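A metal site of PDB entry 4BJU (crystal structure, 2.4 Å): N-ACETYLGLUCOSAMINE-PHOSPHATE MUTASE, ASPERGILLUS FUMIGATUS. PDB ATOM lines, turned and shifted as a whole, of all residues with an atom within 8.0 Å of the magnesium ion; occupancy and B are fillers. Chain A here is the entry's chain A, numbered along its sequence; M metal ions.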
ATOM      1  N   ALA A  30      -0.404 -15.402   7.066  1.00  0.00           N
ATOM      2  CA  ALA A  30      -0.241 -16.097   5.777  1.00  0.00           C
ATOM      3  C   ALA A  30      -1.150 -17.337   5.590  1.00  0.00           C
ATOM      4  O   ALA A  30      -1.110 -17.993   4.539  1.00  0.00           O
ATOM      5  CB  ALA A  30       1.223 -16.452   5.539  1.00  0.00           C
ATOM      6  N   ARG A  33      -0.722 -23.466   6.507  1.00  0.00           N
ATOM      7  CA  ARG A  33       0.585 -23.825   5.987  1.00  0.00           C
ATOM      8  C   ARG A  33       1.149 -25.035   6.749  1.00  0.00           C
ATOM      9  O   ARG A  33       1.318 -24.974   7.966  1.00  0.00           O
ATOM     10  CB  ARG A  33       1.545 -22.644   6.110  1.00  0.00           C
ATOM     11  CG  ARG A  33       2.792 -22.776   5.233  1.00  0.00           C
ATOM     12  CD  ARG A  33       3.627 -21.513   5.290  1.00  0.00           C
ATOM     13  NE  ARG A  33       3.058 -20.457   4.469  1.00  0.00           N
ATOM     14  CZ  ARG A  33       3.606 -19.270   4.284  1.00  0.00           C
ATOM     15  NH1 ARG A  33       4.764 -18.956   4.858  1.00  0.00           N
ATOM     16  NH2 ARG A  33       2.990 -18.375   3.516  1.00  0.00           N
ATOM     17  N   THR A  67       0.541 -21.250  -1.808  1.00  0.00           N
ATOM     18  CA  THR A  67       1.992 -21.183  -1.673  1.00  0.00           C
ATOM     19  C   THR A  67       2.347 -21.468  -0.227  1.00  0.00           C
ATOM     20  O   THR A  67       1.507 -21.270   0.655  1.00  0.00           O
ATOM     21  CB  THR A  67       2.585 -19.792  -2.049  1.00  0.00           C
ATOM     22  OG1 THR A  67       4.020 -19.884  -2.080  1.00  0.00           O
ATOM     23  CG2 THR A  67       2.206 -18.714  -1.051  1.00  0.00           C
ATOM     24  N   ALA A  68       3.588 -21.893   0.011  1.00  0.00           N
ATOM     25  CA  ALA A  68       4.124 -21.971   1.361  1.00  0.00           C
ATOM     26  C   ALA A  68       5.412 -21.165   1.484  1.00  0.00           C
ATOM     27  O   ALA A  68       6.170 -21.338   2.431  1.00  0.00           O
ATOM     28  CB  ALA A  68       4.328 -23.423   1.789  1.00  0.00           C
ATOM     29  N   SEP A  69       5.665 -20.278   0.520  1.00  0.00           N
ATOM     30  CA  SEP A  69       6.736 -19.293   0.617  1.00  0.00           C
ATOM     31  CB  SEP A  69       6.357 -18.389   1.787  1.00  0.00           C
ATOM     32  OG  SEP A  69       7.203 -17.256   1.795  1.00  0.00           O
ATOM     33  C   SEP A  69       8.131 -19.899   0.730  1.00  0.00           C
ATOM     34  O   SEP A  69       8.572 -20.519  -0.245  1.00  0.00           O
ATOM     35  P   SEP A  69       7.381 -16.447   3.168  1.00  0.00           P
ATOM     36  O1P SEP A  69       8.682 -17.001   3.724  1.00  0.00           O
ATOM     37  O2P SEP A  69       7.363 -15.002   2.646  1.00  0.00           O
ATOM     38  O3P SEP A  69       6.228 -16.827   4.072  1.00  0.00           O
ATOM     39  N   HIS A  70       8.817 -19.715   1.890  1.00  0.00           N
ATOM     40  CA  HIS A  70      10.198 -20.205   2.193  1.00  0.00           C
ATOM     41  C   HIS A  70      10.282 -21.710   2.302  1.00  0.00           C
ATOM     42  O   HIS A  70      11.357 -22.280   2.154  1.00  0.00           O
ATOM     43  CB  HIS A  70      10.844 -19.467   3.434  1.00  0.00           C
ATOM     44  CG  HIS A  70      10.931 -20.253   4.756  1.00  0.00           C
ATOM     45  ND1 HIS A  70      10.108 -19.978   5.836  1.00  0.00           N
ATOM     46  CD2 HIS A  70      11.811 -21.194   5.205  1.00  0.00           C
ATOM     47  CE1 HIS A  70      10.443 -20.758   6.862  1.00  0.00           C
ATOM     48  NE2 HIS A  70      11.481 -21.508   6.514  1.00  0.00           N
ATOM     49  N   ASN A  71       9.138 -22.345   2.571  1.00  0.00           N
ATOM     50  CA  ASN A  71       9.102 -23.729   3.045  1.00  0.00           C
ATOM     51  C   ASN A  71       9.538 -24.744   1.994  1.00  0.00           C
ATOM     52  O   ASN A  71       9.430 -24.461   0.792  1.00  0.00           O
ATOM     53  CB  ASN A  71       7.690 -24.072   3.538  1.00  0.00           C
ATOM     54  CG  ASN A  71       7.337 -23.408   4.870  1.00  0.00           C
ATOM     55  OD1 ASN A  71       7.978 -22.438   5.303  1.00  0.00           O
ATOM     56  ND2 ASN A  71       6.294 -23.913   5.516  1.00  0.00           N
ATOM     57  N   THR A 164       3.191 -14.211  -5.324  1.00  0.00           N
ATOM     58  CA  THR A 164       2.200 -13.704  -4.372  1.00  0.00           C
ATOM     59  C   THR A 164       1.811 -12.221  -4.645  1.00  0.00           C
ATOM     60  O   THR A 164       0.611 -11.892  -4.714  1.00  0.00           O
ATOM     61  CB  THR A 164       2.644 -13.928  -2.910  1.00  0.00           C
ATOM     62  OG1 THR A 164       2.553 -15.320  -2.584  1.00  0.00           O
ATOM     63  CG2 THR A 164       1.795 -13.137  -1.937  1.00  0.00           C
ATOM     64  N   PRO A 165       2.794 -11.321  -4.845  1.00  0.00           N
ATOM     65  CA  PRO A 165       2.422  -9.943  -5.116  1.00  0.00           C
ATOM     66  C   PRO A 165       1.577  -9.767  -6.380  1.00  0.00           C
ATOM     67  O   PRO A 165       0.715  -8.900  -6.399  1.00  0.00           O
ATOM     68  CB  PRO A 165       3.775  -9.231  -5.278  1.00  0.00           C
ATOM     69  CG  PRO A 165       4.722 -10.071  -4.507  1.00  0.00           C
ATOM     70  CD  PRO A 165       4.250 -11.478  -4.689  1.00  0.00           C
ATOM     71  N   ASN A 254      13.618 -23.612  -3.045  1.00  0.00           N
ATOM     72  CA  ASN A 254      14.172 -23.172  -1.760  1.00  0.00           C
ATOM     73  C   ASN A 254      15.301 -24.072  -1.215  1.00  0.00           C
ATOM     74  O   ASN A 254      15.699 -23.929  -0.070  1.00  0.00           O
ATOM     75  CB  ASN A 254      13.054 -23.016  -0.711  1.00  0.00           C
ATOM     76  CG  ASN A 254      11.995 -22.003  -1.128  1.00  0.00           C
ATOM     77  OD1 ASN A 254      12.324 -20.901  -1.581  1.00  0.00           O
ATOM     78  ND2 ASN A 254      10.721 -22.379  -0.988  1.00  0.00           N
ATOM     79  N   ALA A 259      16.097 -16.396  -0.523  1.00  0.00           N
ATOM     80  CA  ALA A 259      16.122 -15.317   0.480  1.00  0.00           C
ATOM     81  C   ALA A 259      16.144 -15.766   1.938  1.00  0.00           C
ATOM     82  O   ALA A 259      17.006 -15.341   2.717  1.00  0.00           O
ATOM     83  CB  ALA A 259      15.036 -14.273   0.233  1.00  0.00           C
ATOM     84  N   ASP A 260      15.212 -16.632   2.322  1.00  0.00           N
ATOM     85  CA  ASP A 260      15.208 -17.147   3.680  1.00  0.00           C
ATOM     86  C   ASP A 260      16.535 -17.871   4.031  1.00  0.00           C
ATOM     87  O   ASP A 260      17.054 -17.713   5.134  1.00  0.00           O
ATOM     88  CB  ASP A 260      13.984 -18.033   3.906  1.00  0.00           C
ATOM     89  CG  ASP A 260      13.855 -18.459   5.343  1.00  0.00           C
ATOM     90  OD1 ASP A 260      14.483 -19.472   5.710  1.00  0.00           O
ATOM     91  OD2 ASP A 260      13.128 -17.781   6.098  1.00  0.00           O
ATOM     92  N   LEU A 283      15.516 -13.708  -3.996  1.00  0.00           N
ATOM     93  CA  LEU A 283      14.073 -13.722  -3.841  1.00  0.00           C
ATOM     94  C   LEU A 283      13.699 -14.932  -2.983  1.00  0.00           C
ATOM     95  O   LEU A 283      14.433 -15.930  -2.998  1.00  0.00           O
ATOM     96  CB  LEU A 283      13.410 -13.911  -5.214  1.00  0.00           C
ATOM     97  CG  LEU A 283      13.781 -12.948  -6.346  1.00  0.00           C
ATOM     98  CD1 LEU A 283      12.809 -13.117  -7.499  1.00  0.00           C
ATOM     99  CD2 LEU A 283      13.811 -11.509  -5.882  1.00  0.00           C
ATOM    100  N   ASP A 284      12.573 -14.875  -2.263  1.00  0.00           N
ATOM    101  CA  ASP A 284      12.055 -16.131  -1.677  1.00  0.00           C
ATOM    102  C   ASP A 284      11.185 -16.863  -2.708  1.00  0.00           C
ATOM    103  O   ASP A 284      10.972 -16.352  -3.820  1.00  0.00           O
ATOM    104  CB  ASP A 284      11.263 -15.885  -0.388  1.00  0.00           C
ATOM    105  CG  ASP A 284       9.910 -15.191  -0.612  1.00  0.00           C
ATOM    106  OD1 ASP A 284       9.780 -14.454  -1.630  1.00  0.00           O
ATOM    107  OD2 ASP A 284       8.995 -15.354   0.257  1.00  0.00           O
ATOM    108  N   GLY A 285      10.669 -18.015  -2.314  1.00  0.00           N
ATOM    109  CA  GLY A 285       9.945 -18.924  -3.219  1.00  0.00           C
ATOM    110  C   GLY A 285       8.636 -18.437  -3.844  1.00  0.00           C
ATOM    111  O   GLY A 285       8.221 -18.967  -4.870  1.00  0.00           O
ATOM    112  N   ASP A 286       7.990 -17.438  -3.246  1.00  0.00           N
ATOM    113  CA  ASP A 286       6.775 -16.836  -3.810  1.00  0.00           C
ATOM    114  C   ASP A 286       7.007 -15.361  -4.103  1.00  0.00           C
ATOM    115  O   ASP A 286       6.079 -14.624  -4.439  1.00  0.00           O
ATOM    116  CB  ASP A 286       5.558 -17.032  -2.894  1.00  0.00           C
ATOM    117  CG  ASP A 286       5.670 -16.272  -1.570  1.00  0.00           C
ATOM    118  OD1 ASP A 286       6.774 -16.046  -0.980  1.00  0.00           O
ATOM    119  OD2 ASP A 286       4.578 -15.938  -1.068  1.00  0.00           O
ATOM    120  N   ALA A 287       8.265 -14.975  -3.994  1.00  0.00           N
ATOM    121  CA  ALA A 287       8.767 -13.667  -4.391  1.00  0.00           C
ATOM    122  C   ALA A 287       8.103 -12.470  -3.714  1.00  0.00           C
ATOM    123  O   ALA A 287       7.842 -11.464  -4.360  1.00  0.00           O
ATOM    124  CB  ALA A 287       8.764 -13.524  -5.922  1.00  0.00           C
ATOM    125  N   ASP A 288       7.871 -12.570  -2.393  1.00  0.00           N
ATOM    126  CA  ASP A 288       7.428 -11.409  -1.611  1.00  0.00           C
ATOM    127  C   ASP A 288       8.509 -10.942  -0.638  1.00  0.00           C
ATOM    128  O   ASP A 288       8.290 -10.022   0.153  1.00  0.00           O
ATOM    129  CB  ASP A 288       6.105 -11.697  -0.868  1.00  0.00           C
ATOM    130  CG  ASP A 288       6.236 -12.773   0.173  1.00  0.00           C
ATOM    131  OD1 ASP A 288       7.195 -13.585   0.123  1.00  0.00           O
ATOM    132  OD2 ASP A 288       5.356 -12.811   1.055  1.00  0.00           O
ATOM    133  N   ARG A 289       9.679 -11.578  -0.708  1.00  0.00           N
ATOM    134  CA  ARG A 289      10.837 -11.198   0.086  1.00  0.00           C
ATOM    135  C   ARG A 289      12.092 -11.086  -0.792  1.00  0.00           C
ATOM    136  O   ARG A 289      12.297 -11.852  -1.719  1.00  0.00           O
ATOM    137  CB  ARG A 289      11.079 -12.238   1.217  1.00  0.00           C
ATOM    138  CG  ARG A 289      10.002 -12.307   2.294  1.00  0.00           C
ATOM    139  CD  ARG A 289      10.047 -13.623   3.081  1.00  0.00           C
ATOM    140  NE  ARG A 289      11.356 -13.800   3.689  1.00  0.00           N
ATOM    141  CZ  ARG A 289      11.829 -14.919   4.258  1.00  0.00           C
ATOM    142  NH1 ARG A 289      11.110 -16.039   4.309  1.00  0.00           N
ATOM    143  NH2 ARG A 289      13.038 -14.894   4.786  1.00  0.00           N
ATOM    144  N   ILE A 290      12.979 -10.164  -0.456  1.00  0.00           N
ATOM    145  CA  ILE A 290      14.253 -10.038  -1.146  1.00  0.00           C
ATOM    146  C   ILE A 290      15.340  -9.532  -0.208  1.00  0.00           C
ATOM    147  O   ILE A 290      15.093  -8.671   0.638  1.00  0.00           O
ATOM    148  CB  ILE A 290      14.149  -9.057  -2.356  1.00  0.00           C
ATOM    149  CG1 ILE A 290      15.469  -8.898  -3.099  1.00  0.00           C
ATOM    150  CG2 ILE A 290      13.684  -7.672  -1.926  1.00  0.00           C
ATOM    151  CD1 ILE A 290      15.307  -8.248  -4.466  1.00  0.00           C
ATOM    152  N   HIS A 384      10.894  -8.686   3.682  1.00  0.00           N
ATOM    153  CA  HIS A 384       9.522  -8.304   3.400  1.00  0.00           C
ATOM    154  C   HIS A 384       9.272  -6.838   3.753  1.00  0.00           C
ATOM    155  O   HIS A 384       9.521  -6.419   4.874  1.00  0.00           O
ATOM    156  CB  HIS A 384       8.497  -9.192   4.104  1.00  0.00           C
ATOM    157  CG  HIS A 384       7.093  -9.010   3.598  1.00  0.00           C
ATOM    158  ND1 HIS A 384       6.684  -9.455   2.355  1.00  0.00           N
ATOM    159  CD2 HIS A 384       6.020  -8.399   4.152  1.00  0.00           C
ATOM    160  CE1 HIS A 384       5.413  -9.140   2.174  1.00  0.00           C
ATOM    161  NE2 HIS A 384       4.987  -8.499   3.248  1.00  0.00           N
ATOM    162  N   GLY A 426       4.269  -6.254   0.164  1.00  0.00           N
ATOM    163  CA  GLY A 426       5.702  -6.309  -0.106  1.00  0.00           C
ATOM    164  C   GLY A 426       5.988  -7.204  -1.295  1.00  0.00           C
ATOM    165  O   GLY A 426       5.488  -8.323  -1.377  1.00  0.00           O
ATOM    166  N   ALA A 428       8.963  -8.475  -3.911  1.00  0.00           N
ATOM    167  CA  ALA A 428      10.380  -8.673  -4.133  1.00  0.00           C
ATOM    168  C   ALA A 428      10.840  -8.018  -5.440  1.00  0.00           C
ATOM    169  O   ALA A 428      11.877  -7.313  -5.480  1.00  0.00           O
ATOM    170  CB  ALA A 428      10.688 -10.150  -4.139  1.00  0.00           C
HETATM  171 MG    MG M   1       7.181 -15.325   0.760  1.00  0.00          MG
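A ring nitrogen (ND1) of His 384 is in hydrogen-bond range of the backbone carbonyl oxygen (O) of Asp 288. O1P of SEP 69 is in salt-bridge range of the guanidinium group (NH1) of Arg 289 (2.7 Å). The backbone NH (N) of Ala 287 lies within hydrogen-bond range of the side-chain carboxylate (OD1) of Asp 284. OD2 of Asp 286 sits at hydrogen-bond distance from OG1 of Thr 164, 2.6 Å away. O3P of SEP 69 is in salt-bridge range of the guanidinium group (NH1) of Arg 33, at 2.7 Å. The side-chain carboxylate of Asp 284 is in hydrogen-bond range of the backbone NH of Arg 289. The side-chain amide nitrogen (ND2) of Asn 254 is in hydrogen-bond range of O of SEP 69 (2.9 Å). OG1 of Thr 67 sits at hydrogen-bond distance from N of SEP 69 (3.1 Å).
Four residues have an atom within 4 Å of the magnesium ion: SEP 69, Asp 284, Asp 286 and Asp 288.
The magnesium ion is bound by the side-chain carboxylate of Asp 288, the side-chain carboxylate of Asp 284, O2P of SEP 69, the side-chain carboxylate of Asp 286 and OG of SEP 69.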
